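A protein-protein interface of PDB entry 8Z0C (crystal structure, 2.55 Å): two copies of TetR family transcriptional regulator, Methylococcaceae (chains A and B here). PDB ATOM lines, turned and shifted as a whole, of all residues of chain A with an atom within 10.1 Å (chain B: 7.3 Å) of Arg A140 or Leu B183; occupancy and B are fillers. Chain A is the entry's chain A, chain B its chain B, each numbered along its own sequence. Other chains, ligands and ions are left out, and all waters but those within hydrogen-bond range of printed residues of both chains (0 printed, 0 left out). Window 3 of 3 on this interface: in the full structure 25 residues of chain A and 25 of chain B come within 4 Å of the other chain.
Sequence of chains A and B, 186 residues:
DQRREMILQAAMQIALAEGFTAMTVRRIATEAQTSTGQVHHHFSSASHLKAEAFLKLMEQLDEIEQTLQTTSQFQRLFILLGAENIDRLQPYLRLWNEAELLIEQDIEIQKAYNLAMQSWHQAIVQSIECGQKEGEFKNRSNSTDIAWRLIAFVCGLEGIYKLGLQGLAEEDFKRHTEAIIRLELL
The guanidinium group (NE) of Arg A149 is in salt-bridge range of the side-chain carboxylate (OE2) of Glu A184, at 2.7 Å.
O of Leu B183 lies within hydrogen-bond range of NH1 of Arg B140 (2.5 Å).
Among the printed residues, pairs that only touch across the chains: Arg A140 with Leu B183 (3.3 Å), Asp A145 with His B176 (3.4 Å), Arg A149 with Ala B179 (3.8 Å), Arg A149 with Ile B180 (3.7 Å), Ile A180 with Glu B184 (3.6 Å), Leu A183 with Leu B183 (3.1 Å), Leu A183 with Glu B184 (3.6 Å), Glu A184 with Ile B180 (3.9 Å) and Glu A184 with Leu B183 (3.9 Å).
Arg A140 touches Leu B183, but with the chains exchanged Leu A183 does not touch Arg B140 (4.7 Å).
Ile A180 touches Glu B184, and with the chains exchanged Glu A184 touches Ile B180.
Leu A183 touches its own counterpart, Leu B183.
Leu A183 touches Glu B184, and with the chains exchanged Glu A184 touches Leu B183.
Of the 10 pairs that touch across the chains among the printed residues, 5 have their exchanged pair printed and touching as well.
Printed residues of chain B within 4 Å of Arg A140: Leu B183 (3.3 Å).
Of chain A, only Arg A140, Leu A183 and Glu A184 come within 4 Å of Leu B183.
Of chain A, only Arg A149 (3.8 Å) comes within 4 Å of Ala B179.
Ile B180 touches just these residues of chain A: Arg A149 (3.7 Å) and Glu A184 (3.9 Å).
Of the printed residues of chain A, His B176 touches Asp A145 (3.4 Å) and Arg A149 (3.0 Å).
Printed residues of chain B within 4 Å of Glu A184: Ile B180 (3.9 Å) and Leu B183 (3.9 Å).
NH1 of Arg A149 sits at hydrogen-bond distance from ND1 of His B176 (3.0 Å).
Hydrophobic or aromatic side chains of chain A within 4 Å of the printed part of chain B: Ile A180 and Leu A183.
Printed residues of chain B that touch a printed residue of chain A: His B176, Ala B179, Ile B180, Leu B183 and Glu B184.
Among the printed residues, 10 pairs touch across the chains.
Among the printed residues, no Asp or Glu carboxylate lies within 4 Å of a Lys or Arg side-chain nitrogen of the other chain.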
ATOM      1  N   ILE A 128      30.247   2.895  -0.239  1.00  0.00           N
ATOM      2  CA  ILE A 128      30.030   1.505  -0.634  1.00  0.00           C
ATOM      3  C   ILE A 128      30.842   1.193  -1.882  1.00  0.00           C
ATOM      4  O   ILE A 128      31.676   0.279  -1.895  1.00  0.00           O
ATOM      5  CB  ILE A 128      28.532   1.244  -0.871  1.00  0.00           C
ATOM      6  CG1 ILE A 128      27.734   1.314   0.443  1.00  0.00           C
ATOM      7  CG2 ILE A 128      28.311  -0.075  -1.618  1.00  0.00           C
ATOM      8  CD1 ILE A 128      26.332   1.827   0.239  1.00  0.00           C
ATOM      9  N   GLY A 131      34.586   1.065  -1.204  1.00  0.00           N
ATOM     10  CA  GLY A 131      35.002  -0.170  -0.570  1.00  0.00           C
ATOM     11  C   GLY A 131      34.899  -1.356  -1.509  1.00  0.00           C
ATOM     12  O   GLY A 131      35.688  -2.301  -1.416  1.00  0.00           O
ATOM     13  N   GLN A 132      33.937  -1.315  -2.433  1.00  0.00           N
ATOM     14  CA  GLN A 132      33.752  -2.418  -3.362  1.00  0.00           C
ATOM     15  C   GLN A 132      34.883  -2.448  -4.385  1.00  0.00           C
ATOM     16  O   GLN A 132      35.492  -3.496  -4.617  1.00  0.00           O
ATOM     17  CB  GLN A 132      32.378  -2.309  -4.036  1.00  0.00           C
ATOM     18  CG  GLN A 132      31.238  -2.810  -3.168  1.00  0.00           C
ATOM     19  CD  GLN A 132      29.885  -2.571  -3.798  1.00  0.00           C
ATOM     20  OE1 GLN A 132      29.785  -1.876  -4.809  1.00  0.00           O
ATOM     21  NE2 GLN A 132      28.832  -3.150  -3.212  1.00  0.00           N
ATOM     22  N   GLU A 136      37.329  -4.288  -0.097  1.00  0.00           N
ATOM     23  CA  GLU A 136      36.902  -4.334   1.299  1.00  0.00           C
ATOM     24  C   GLU A 136      35.478  -4.864   1.467  1.00  0.00           C
ATOM     25  O   GLU A 136      35.225  -5.650   2.382  1.00  0.00           O
ATOM     26  CB  GLU A 136      37.038  -2.945   1.938  1.00  0.00           C
ATOM     27  CG  GLU A 136      38.311  -2.217   1.525  1.00  0.00           C
ATOM     28  CD  GLU A 136      38.609  -0.972   2.359  1.00  0.00           C
ATOM     29  OE1 GLU A 136      39.215  -1.125   3.447  1.00  0.00           O
ATOM     30  OE2 GLU A 136      38.250   0.157   1.915  1.00  0.00           O
ATOM     31  N   PHE A 137      34.543  -4.449   0.617  1.00  0.00           N
ATOM     32  CA  PHE A 137      33.163  -4.920   0.639  1.00  0.00           C
ATOM     33  C   PHE A 137      32.943  -5.823  -0.568  1.00  0.00           C
ATOM     34  O   PHE A 137      33.638  -5.702  -1.578  1.00  0.00           O
ATOM     35  CB  PHE A 137      32.133  -3.758   0.580  1.00  0.00           C
ATOM     36  CG  PHE A 137      32.306  -2.683   1.641  1.00  0.00           C
ATOM     37  CD1 PHE A 137      32.702  -2.987   2.937  1.00  0.00           C
ATOM     38  CD2 PHE A 137      32.044  -1.356   1.332  1.00  0.00           C
ATOM     39  CE1 PHE A 137      32.845  -1.983   3.899  1.00  0.00           C
ATOM     40  CE2 PHE A 137      32.174  -0.339   2.300  1.00  0.00           C
ATOM     41  CZ  PHE A 137      32.575  -0.653   3.575  1.00  0.00           C
ATOM     42  N   LYS A 138      31.948  -6.703  -0.483  1.00  0.00           N
ATOM     43  CA  LYS A 138      31.551  -7.445  -1.669  1.00  0.00           C
ATOM     44  C   LYS A 138      30.410  -6.749  -2.403  1.00  0.00           C
ATOM     45  O   LYS A 138      29.793  -5.800  -1.905  1.00  0.00           O
ATOM     46  CB  LYS A 138      31.166  -8.888  -1.331  1.00  0.00           C
ATOM     47  CG  LYS A 138      30.118  -9.054  -0.232  1.00  0.00           C
ATOM     48  CD  LYS A 138      30.414 -10.331   0.585  1.00  0.00           C
ATOM     49  CE  LYS A 138      29.155 -11.003   1.213  1.00  0.00           C
ATOM     50  NZ  LYS A 138      27.997 -10.116   1.539  1.00  0.00           N
ATOM     51  N   ASN A 139      30.170  -7.208  -3.628  1.00  0.00           N
ATOM     52  CA  ASN A 139      29.178  -6.605  -4.515  1.00  0.00           C
ATOM     53  C   ASN A 139      27.924  -7.468  -4.556  1.00  0.00           C
ATOM     54  O   ASN A 139      27.518  -7.987  -5.582  1.00  0.00           O
ATOM     55  CB  ASN A 139      29.758  -6.391  -5.914  1.00  0.00           C
ATOM     56  CG  ASN A 139      29.076  -5.244  -6.653  1.00  0.00           C
ATOM     57  OD1 ASN A 139      27.889  -4.963  -6.430  1.00  0.00           O
ATOM     58  ND2 ASN A 139      29.833  -4.542  -7.498  1.00  0.00           N
ATOM     59  N   ARG A 140      27.308  -7.595  -3.386  1.00  0.00           N
ATOM     60  CA  ARG A 140      26.098  -8.393  -3.263  1.00  0.00           C
ATOM     61  C   ARG A 140      24.928  -7.742  -3.993  1.00  0.00           C
ATOM     62  O   ARG A 140      24.038  -8.437  -4.500  1.00  0.00           O
ATOM     63  CB  ARG A 140      25.765  -8.570  -1.783  1.00  0.00           C
ATOM     64  CG  ARG A 140      26.280  -9.818  -1.111  1.00  0.00           C
ATOM     65  CD  ARG A 140      25.292 -10.234  -0.025  1.00  0.00           C
ATOM     66  NE  ARG A 140      23.876 -10.224  -0.470  1.00  0.00           N
ATOM     67  CZ  ARG A 140      23.231 -11.268  -1.009  1.00  0.00           C
ATOM     68  NH1 ARG A 140      23.873 -12.418  -1.200  1.00  0.00           N
ATOM     69  NH2 ARG A 140      21.952 -11.160  -1.364  1.00  0.00           N
ATOM     70  N   SER A 141      24.887  -6.410  -4.029  1.00  0.00           N
ATOM     71  CA  SER A 141      23.693  -5.724  -4.512  1.00  0.00           C
ATOM     72  C   SER A 141      24.057  -4.334  -5.030  1.00  0.00           C
ATOM     73  O   SER A 141      25.168  -3.833  -4.826  1.00  0.00           O
ATOM     74  CB  SER A 141      22.628  -5.648  -3.409  1.00  0.00           C
ATOM     75  OG  SER A 141      21.543  -4.804  -3.780  1.00  0.00           O
ATOM     76  N   ASN A 142      23.102  -3.737  -5.739  1.00  0.00           N
ATOM     77  CA  ASN A 142      23.187  -2.337  -6.132  1.00  0.00           C
ATOM     78  C   ASN A 142      23.589  -1.466  -4.935  1.00  0.00           C
ATOM     79  O   ASN A 142      23.059  -1.624  -3.832  1.00  0.00           O
ATOM     80  CB  ASN A 142      21.821  -1.924  -6.708  1.00  0.00           C
ATOM     81  CG  ASN A 142      21.768  -0.471  -7.151  1.00  0.00           C
ATOM     82  OD1 ASN A 142      22.793   0.215  -7.248  1.00  0.00           O
ATOM     83  ND2 ASN A 142      20.560   0.008  -7.427  1.00  0.00           N
ATOM     84  N   SER A 143      24.551  -0.560  -5.147  1.00  0.00           N
ATOM     85  CA  SER A 143      25.058   0.267  -4.053  1.00  0.00           C
ATOM     86  C   SER A 143      24.048   1.328  -3.610  1.00  0.00           C
ATOM     87  O   SER A 143      24.115   1.820  -2.474  1.00  0.00           O
ATOM     88  CB  SER A 143      26.339   0.953  -4.486  1.00  0.00           C
ATOM     89  OG  SER A 143      26.042   1.832  -5.556  1.00  0.00           O
ATOM     90  N   THR A 144      23.148   1.735  -4.506  1.00  0.00           N
ATOM     91  CA  THR A 144      22.113   2.687  -4.143  1.00  0.00           C
ATOM     92  C   THR A 144      21.032   2.017  -3.312  1.00  0.00           C
ATOM     93  O   THR A 144      20.408   2.660  -2.463  1.00  0.00           O
ATOM     94  CB  THR A 144      21.524   3.296  -5.411  1.00  0.00           C
ATOM     95  OG1 THR A 144      22.569   3.973  -6.114  1.00  0.00           O
ATOM     96  CG2 THR A 144      20.407   4.287  -5.090  1.00  0.00           C
ATOM     97  N   ASP A 145      20.811   0.724  -3.537  1.00  0.00           N
ATOM     98  CA  ASP A 145      19.860  -0.020  -2.724  1.00  0.00           C
ATOM     99  C   ASP A 145      20.422  -0.285  -1.331  1.00  0.00           C
ATOM    100  O   ASP A 145      19.719  -0.121  -0.326  1.00  0.00           O
ATOM    101  CB  ASP A 145      19.488  -1.328  -3.432  1.00  0.00           C
ATOM    102  CG  ASP A 145      18.498  -1.114  -4.576  1.00  0.00           C
ATOM    103  OD1 ASP A 145      17.884  -0.019  -4.641  1.00  0.00           O
ATOM    104  OD2 ASP A 145      18.323  -2.038  -5.402  1.00  0.00           O
ATOM    105  N   ILE A 146      21.686  -0.700  -1.246  1.00  0.00           N
ATOM    106  CA  ILE A 146      22.325  -0.873   0.055  1.00  0.00           C
ATOM    107  C   ILE A 146      22.242   0.423   0.854  1.00  0.00           C
ATOM    108  O   ILE A 146      21.842   0.436   2.025  1.00  0.00           O
ATOM    109  CB  ILE A 146      23.789  -1.318  -0.119  1.00  0.00           C
ATOM    110  CG1 ILE A 146      23.911  -2.511  -1.087  1.00  0.00           C
ATOM    111  CG2 ILE A 146      24.444  -1.552   1.255  1.00  0.00           C
ATOM    112  CD1 ILE A 146      23.577  -3.846  -0.511  1.00  0.00           C
ATOM    113  N   ARG A 149      18.946   1.297   2.130  1.00  0.00           N
ATOM    114  CA  ARG A 149      18.537   0.417   3.212  1.00  0.00           C
ATOM    115  C   ARG A 149      19.363   0.637   4.472  1.00  0.00           C
ATOM    116  O   ARG A 149      18.853   0.444   5.577  1.00  0.00           O
ATOM    117  CB  ARG A 149      18.618  -1.036   2.762  1.00  0.00           C
ATOM    118  CG  ARG A 149      17.569  -1.391   1.725  1.00  0.00           C
ATOM    119  CD  ARG A 149      17.473  -2.881   1.521  1.00  0.00           C
ATOM    120  NE  ARG A 149      18.726  -3.471   1.068  1.00  0.00           N
ATOM    121  CZ  ARG A 149      18.939  -3.896  -0.177  1.00  0.00           C
ATOM    122  NH1 ARG A 149      17.988  -3.765  -1.095  1.00  0.00           N
ATOM    123  NH2 ARG A 149      20.100  -4.462  -0.508  1.00  0.00           N
ATOM    124  N   LEU A 150      20.630   1.023   4.345  1.00  0.00           N
ATOM    125  CA  LEU A 150      21.381   1.382   5.546  1.00  0.00           C
ATOM    126  C   LEU A 150      20.803   2.652   6.192  1.00  0.00           C
ATOM    127  O   LEU A 150      20.720   2.750   7.420  1.00  0.00           O
ATOM    128  CB  LEU A 150      22.874   1.549   5.216  1.00  0.00           C
ATOM    129  CG  LEU A 150      23.678   0.444   4.511  1.00  0.00           C
ATOM    130  CD1 LEU A 150      25.156   0.827   4.386  1.00  0.00           C
ATOM    131  CD2 LEU A 150      23.546  -0.930   5.172  1.00  0.00           C
ATOM    132  N   ALA A 179      26.022  -5.239  12.533  1.00  0.00           N
ATOM    133  CA  ALA A 179      25.541  -6.512  12.001  1.00  0.00           C
ATOM    134  C   ALA A 179      24.904  -6.338  10.626  1.00  0.00           C
ATOM    135  O   ALA A 179      25.198  -7.110   9.706  1.00  0.00           O
ATOM    136  CB  ALA A 179      24.566  -7.170  12.978  1.00  0.00           C
ATOM    137  N   ILE A 180      24.026  -5.334  10.462  1.00  0.00           N
ATOM    138  CA  ILE A 180      23.382  -5.112   9.165  1.00  0.00           C
ATOM    139  C   ILE A 180      24.407  -4.696   8.103  1.00  0.00           C
ATOM    140  O   ILE A 180      24.167  -4.860   6.900  1.00  0.00           O
ATOM    141  CB  ILE A 180      22.243  -4.077   9.303  1.00  0.00           C
ATOM    142  CG1 ILE A 180      21.163  -4.592  10.262  1.00  0.00           C
ATOM    143  CG2 ILE A 180      21.559  -3.790   7.954  1.00  0.00           C
ATOM    144  CD1 ILE A 180      20.213  -5.644   9.627  1.00  0.00           C
ATOM    145  N   ILE A 181      25.558  -4.152   8.513  1.00  0.00           N
ATOM    146  CA  ILE A 181      26.584  -3.802   7.534  1.00  0.00           C
ATOM    147  C   ILE A 181      27.284  -5.058   7.027  1.00  0.00           C
ATOM    148  O   ILE A 181      27.534  -5.200   5.824  1.00  0.00           O
ATOM    149  CB  ILE A 181      27.594  -2.795   8.122  1.00  0.00           C
ATOM    150  CG1 ILE A 181      26.968  -1.419   8.293  1.00  0.00           C
ATOM    151  CG2 ILE A 181      28.825  -2.666   7.218  1.00  0.00           C
ATOM    152  CD1 ILE A 181      27.911  -0.427   8.992  1.00  0.00           C
ATOM    153  N   ARG A 182      27.615  -5.987   7.929  1.00  0.00           N
ATOM    154  CA  ARG A 182      28.250  -7.233   7.493  1.00  0.00           C
ATOM    155  C   ARG A 182      27.345  -8.012   6.558  1.00  0.00           C
ATOM    156  O   ARG A 182      27.816  -8.575   5.562  1.00  0.00           O
ATOM    157  CB  ARG A 182      28.634  -8.098   8.689  1.00  0.00           C
ATOM    158  CG  ARG A 182      29.981  -7.747   9.277  1.00  0.00           C
ATOM    159  CD  ARG A 182      30.021  -8.160  10.732  1.00  0.00           C
ATOM    160  NE  ARG A 182      30.728  -7.195  11.571  1.00  0.00           N
ATOM    161  CZ  ARG A 182      32.048  -7.210  11.749  1.00  0.00           C
ATOM    162  NH1 ARG A 182      32.785  -8.133  11.132  1.00  0.00           N
ATOM    163  NH2 ARG A 182      32.628  -6.309  12.538  1.00  0.00           N
ATOM    164  N   LEU A 183      26.041  -8.051   6.853  1.00  0.00           N
ATOM    165  CA  LEU A 183      25.112  -8.792   6.000  1.00  0.00           C
ATOM    166  C   LEU A 183      25.054  -8.191   4.606  1.00  0.00           C
ATOM    167  O   LEU A 183      25.038  -8.923   3.610  1.00  0.00           O
ATOM    168  CB  LEU A 183      23.711  -8.826   6.616  1.00  0.00           C
ATOM    169  CG  LEU A 183      23.512  -9.608   7.915  1.00  0.00           C
ATOM    170  CD1 LEU A 183      22.031  -9.662   8.248  1.00  0.00           C
ATOM    171  CD2 LEU A 183      24.094 -11.023   7.817  1.00  0.00           C
ATOM    172  N   GLU A 184      25.075  -6.863   4.509  1.00  0.00           N
ATOM    173  CA  GLU A 184      24.900  -6.217   3.213  1.00  0.00           C
ATOM    174  C   GLU A 184      26.193  -6.160   2.405  1.00  0.00           C
ATOM    175  O   GLU A 184      26.147  -6.140   1.174  1.00  0.00           O
ATOM    176  CB  GLU A 184      24.343  -4.796   3.404  1.00  0.00           C
ATOM    177  CG  GLU A 184      22.856  -4.717   3.786  1.00  0.00           C
ATOM    178  CD  GLU A 184      21.933  -4.724   2.569  1.00  0.00           C
ATOM    179  OE1 GLU A 184      22.239  -5.447   1.581  1.00  0.00           O
ATOM    180  OE2 GLU A 184      20.903  -4.011   2.592  1.00  0.00           O
ATOM    181  N   LEU A 185      27.347  -6.135   3.064  1.00  0.00           N
ATOM    182  CA  LEU A 185      28.571  -5.743   2.381  1.00  0.00           C
ATOM    183  C   LEU A 185      29.793  -6.588   2.697  1.00  0.00           C
ATOM    184  O   LEU A 185      30.822  -6.381   2.047  1.00  0.00           O
ATOM    185  CB  LEU A 185      28.900  -4.277   2.716  1.00  0.00           C
ATOM    186  CG  LEU A 185      28.048  -3.177   2.101  1.00  0.00           C
ATOM    187  CD1 LEU A 185      28.168  -1.952   2.985  1.00  0.00           C
ATOM    188  CD2 LEU A 185      28.479  -2.892   0.655  1.00  0.00           C
ATOM    189  N   LEU A 186      29.748  -7.493   3.674  1.00  0.00           N
ATOM    190  CA  LEU A 186      30.939  -8.267   4.052  1.00  0.00           C
ATOM    191  C   LEU A 186      30.711  -9.772   3.990  1.00  0.00           C
ATOM    192  O   LEU A 186      31.551 -10.485   3.463  1.00  0.00           O
ATOM    193  CB  LEU A 186      31.409  -7.905   5.461  1.00  0.00           C
ATOM    194  CG  LEU A 186      32.037  -6.534   5.671  1.00  0.00           C
ATOM    195  CD1 LEU A 186      32.879  -6.529   6.939  1.00  0.00           C
ATOM    196  CD2 LEU A 186      32.856  -6.166   4.453  1.00  0.00           C
ATOM    197  OXT LEU A 186      29.712 -10.323   4.468  1.00  0.00           O
ATOM    198  N   ARG B 140      21.855 -17.826  11.980  1.00  0.00           N
ATOM    199  CA  ARG B 140      23.000 -16.929  12.092  1.00  0.00           C
ATOM    200  C   ARG B 140      22.971 -16.130  13.392  1.00  0.00           C
ATOM    201  O   ARG B 140      24.017 -15.924  14.020  1.00  0.00           O
ATOM    202  CB  ARG B 140      23.038 -15.990  10.891  1.00  0.00           C
ATOM    203  CG  ARG B 140      23.471 -16.679   9.637  1.00  0.00           C
ATOM    204  CD  ARG B 140      23.140 -15.847   8.446  1.00  0.00           C
ATOM    205  NE  ARG B 140      22.610 -16.692   7.389  1.00  0.00           N
ATOM    206  CZ  ARG B 140      22.143 -16.230   6.238  1.00  0.00           C
ATOM    207  NH1 ARG B 140      22.158 -14.923   6.001  1.00  0.00           N
ATOM    208  NH2 ARG B 140      21.686 -17.069   5.322  1.00  0.00           N
ATOM    209  N   HIS B 176      12.723  -4.209  -0.974  1.00  0.00           N
ATOM    210  CA  HIS B 176      13.745  -4.010   0.049  1.00  0.00           C
ATOM    211  C   HIS B 176      13.497  -4.889   1.261  1.00  0.00           C
ATOM    212  O   HIS B 176      14.453  -5.377   1.880  1.00  0.00           O
ATOM    213  CB  HIS B 176      13.807  -2.548   0.447  1.00  0.00           C
ATOM    214  CG  HIS B 176      14.439  -1.679  -0.590  1.00  0.00           C
ATOM    215  ND1 HIS B 176      15.746  -1.843  -1.001  1.00  0.00           N
ATOM    216  CD2 HIS B 176      13.941  -0.656  -1.323  1.00  0.00           C
ATOM    217  CE1 HIS B 176      16.028  -0.952  -1.936  1.00  0.00           C
ATOM    218  NE2 HIS B 176      14.952  -0.215  -2.145  1.00  0.00           N
ATOM    219  N   THR B 177      12.229  -5.133   1.585  1.00  0.00           N
ATOM    220  CA  THR B 177      11.897  -6.080   2.645  1.00  0.00           C
ATOM    221  C   THR B 177      12.331  -7.495   2.280  1.00  0.00           C
ATOM    222  O   THR B 177      12.931  -8.203   3.100  1.00  0.00           O
ATOM    223  CB  THR B 177      10.396  -6.035   2.928  1.00  0.00           C
ATOM    224  OG1 THR B 177       9.975  -4.670   3.002  1.00  0.00           O
ATOM    225  CG2 THR B 177      10.072  -6.749   4.227  1.00  0.00           C
ATOM    226  N   GLU B 178      12.022  -7.931   1.055  1.00  0.00           N
ATOM    227  CA  GLU B 178      12.483  -9.240   0.604  1.00  0.00           C
ATOM    228  C   GLU B 178      13.995  -9.386   0.758  1.00  0.00           C
ATOM    229  O   GLU B 178      14.482 -10.441   1.186  1.00  0.00           O
ATOM    230  CB  GLU B 178      12.067  -9.478  -0.849  1.00  0.00           C
ATOM    231  CG  GLU B 178      12.574 -10.809  -1.420  1.00  0.00           C
ATOM    232  CD  GLU B 178      11.878 -11.190  -2.716  1.00  0.00           C
ATOM    233  OE1 GLU B 178      10.850 -10.545  -3.048  1.00  0.00           O
ATOM    234  OE2 GLU B 178      12.355 -12.127  -3.394  1.00  0.00           O
ATOM    235  N   ALA B 179      14.758  -8.335   0.426  1.00  0.00           N
ATOM    236  CA  ALA B 179      16.207  -8.460   0.516  1.00  0.00           C
ATOM    237  C   ALA B 179      16.651  -8.593   1.962  1.00  0.00           C
ATOM    238  O   ALA B 179      17.477  -9.454   2.281  1.00  0.00           O
ATOM    239  CB  ALA B 179      16.898  -7.282  -0.162  1.00  0.00           C
ATOM    240  N   ILE B 180      16.090  -7.776   2.854  1.00  0.00           N
ATOM    241  CA  ILE B 180      16.484  -7.821   4.260  1.00  0.00           C
ATOM    242  C   ILE B 180      16.205  -9.203   4.858  1.00  0.00           C
ATOM    243  O   ILE B 180      17.063  -9.771   5.552  1.00  0.00           O
ATOM    244  CB  ILE B 180      15.783  -6.687   5.044  1.00  0.00           C
ATOM    245  CG1 ILE B 180      16.174  -5.323   4.478  1.00  0.00           C
ATOM    246  CG2 ILE B 180      16.119  -6.734   6.534  1.00  0.00           C
ATOM    247  CD1 ILE B 180      17.667  -5.072   4.461  1.00  0.00           C
ATOM    248  N   ILE B 181      15.020  -9.778   4.584  1.00  0.00           N
ATOM    249  CA  ILE B 181      14.703 -11.128   5.081  1.00  0.00           C
ATOM    250  C   ILE B 181      15.721 -12.160   4.574  1.00  0.00           C
ATOM    251  O   ILE B 181      16.162 -13.043   5.325  1.00  0.00           O
ATOM    252  CB  ILE B 181      13.264 -11.536   4.695  1.00  0.00           C
ATOM    253  CG1 ILE B 181      12.231 -10.516   5.179  1.00  0.00           C
ATOM    254  CG2 ILE B 181      12.914 -12.908   5.259  1.00  0.00           C
ATOM    255  CD1 ILE B 181      10.949 -10.493   4.342  1.00  0.00           C
ATOM    256  N   ARG B 182      16.108 -12.068   3.299  1.00  0.00           N
ATOM    257  CA  ARG B 182      17.088 -13.006   2.756  1.00  0.00           C
ATOM    258  C   ARG B 182      18.447 -12.867   3.436  1.00  0.00           C
ATOM    259  O   ARG B 182      19.054 -13.869   3.830  1.00  0.00           O
ATOM    260  CB  ARG B 182      17.219 -12.821   1.245  1.00  0.00           C
ATOM    261  CG  ARG B 182      15.986 -13.234   0.472  1.00  0.00           C
ATOM    262  CD  ARG B 182      16.201 -13.132  -1.022  1.00  0.00           C
ATOM    263  NE  ARG B 182      14.943 -13.244  -1.763  1.00  0.00           N
ATOM    264  CZ  ARG B 182      14.333 -14.395  -2.050  1.00  0.00           C
ATOM    265  NH1 ARG B 182      14.858 -15.559  -1.661  1.00  0.00           N
ATOM    266  NH2 ARG B 182      13.187 -14.383  -2.732  1.00  0.00           N
ATOM    267  N   LEU B 183      18.963 -11.640   3.564  1.00  0.00           N
ATOM    268  CA  LEU B 183      20.238 -11.487   4.263  1.00  0.00           C
ATOM    269  C   LEU B 183      20.189 -12.076   5.667  1.00  0.00           C
ATOM    270  O   LEU B 183      21.199 -12.600   6.153  1.00  0.00           O
ATOM    271  CB  LEU B 183      20.654 -10.016   4.359  1.00  0.00           C
ATOM    272  CG  LEU B 183      21.300  -9.296   3.175  1.00  0.00           C
ATOM    273  CD1 LEU B 183      22.382 -10.160   2.515  1.00  0.00           C
ATOM    274  CD2 LEU B 183      20.284  -8.783   2.171  1.00  0.00           C
ATOM    275  N   GLU B 184      19.030 -11.995   6.336  1.00  0.00           N
ATOM    276  CA  GLU B 184      18.961 -12.376   7.743  1.00  0.00           C
ATOM    277  C   GLU B 184      18.770 -13.877   7.930  1.00  0.00           C
ATOM    278  O   GLU B 184      19.406 -14.475   8.805  1.00  0.00           O
ATOM    279  CB  GLU B 184      17.827 -11.620   8.455  1.00  0.00           C
ATOM    280  CG  GLU B 184      18.157 -10.177   8.851  1.00  0.00           C
ATOM    281  CD  GLU B 184      19.030 -10.076  10.110  1.00  0.00           C
ATOM    282  OE1 GLU B 184      19.193  -8.951  10.644  1.00  0.00           O
ATOM    283  OE2 GLU B 184      19.573 -11.119  10.555  1.00  0.00           O
ATOM    284  N   LEU B 185      17.904 -14.500   7.125  1.00  0.00           N
ATOM    285  CA  LEU B 185      17.359 -15.797   7.527  1.00  0.00           C
ATOM    286  C   LEU B 185      17.470 -16.898   6.480  1.00  0.00           C
ATOM    287  O   LEU B 185      17.580 -18.070   6.853  1.00  0.00           O
ATOM    288  CB  LEU B 185      15.880 -15.618   7.927  1.00  0.00           C
ATOM    289  CG  LEU B 185      15.579 -14.700   9.110  1.00  0.00           C
ATOM    290  CD1 LEU B 185      14.129 -14.299   9.039  1.00  0.00           C
ATOM    291  CD2 LEU B 185      15.917 -15.341  10.473  1.00  0.00           C
ATOM    292  N   LEU B 186      17.388 -16.577   5.190  1.00  0.00           N
ATOM    293  CA  LEU B 186      17.579 -17.613   4.162  1.00  0.00           C
ATOM    294  C   LEU B 186      19.058 -17.710   3.806  1.00  0.00           C
ATOM    295  O   LEU B 186      19.679 -18.783   3.852  1.00  0.00           O
ATOM    296  CB  LEU B 186      16.771 -17.340   2.883  1.00  0.00           C
ATOM    297  CG  LEU B 186      15.265 -17.089   2.885  1.00  0.00           C
ATOM    298  CD1 LEU B 186      14.641 -17.557   1.571  1.00  0.00           C
ATOM    299  CD2 LEU B 186      14.599 -17.761   4.053  1.00  0.00           C
ATOM    300  OXT LEU B 186      19.672 -16.695   3.461  1.00  0.00           O
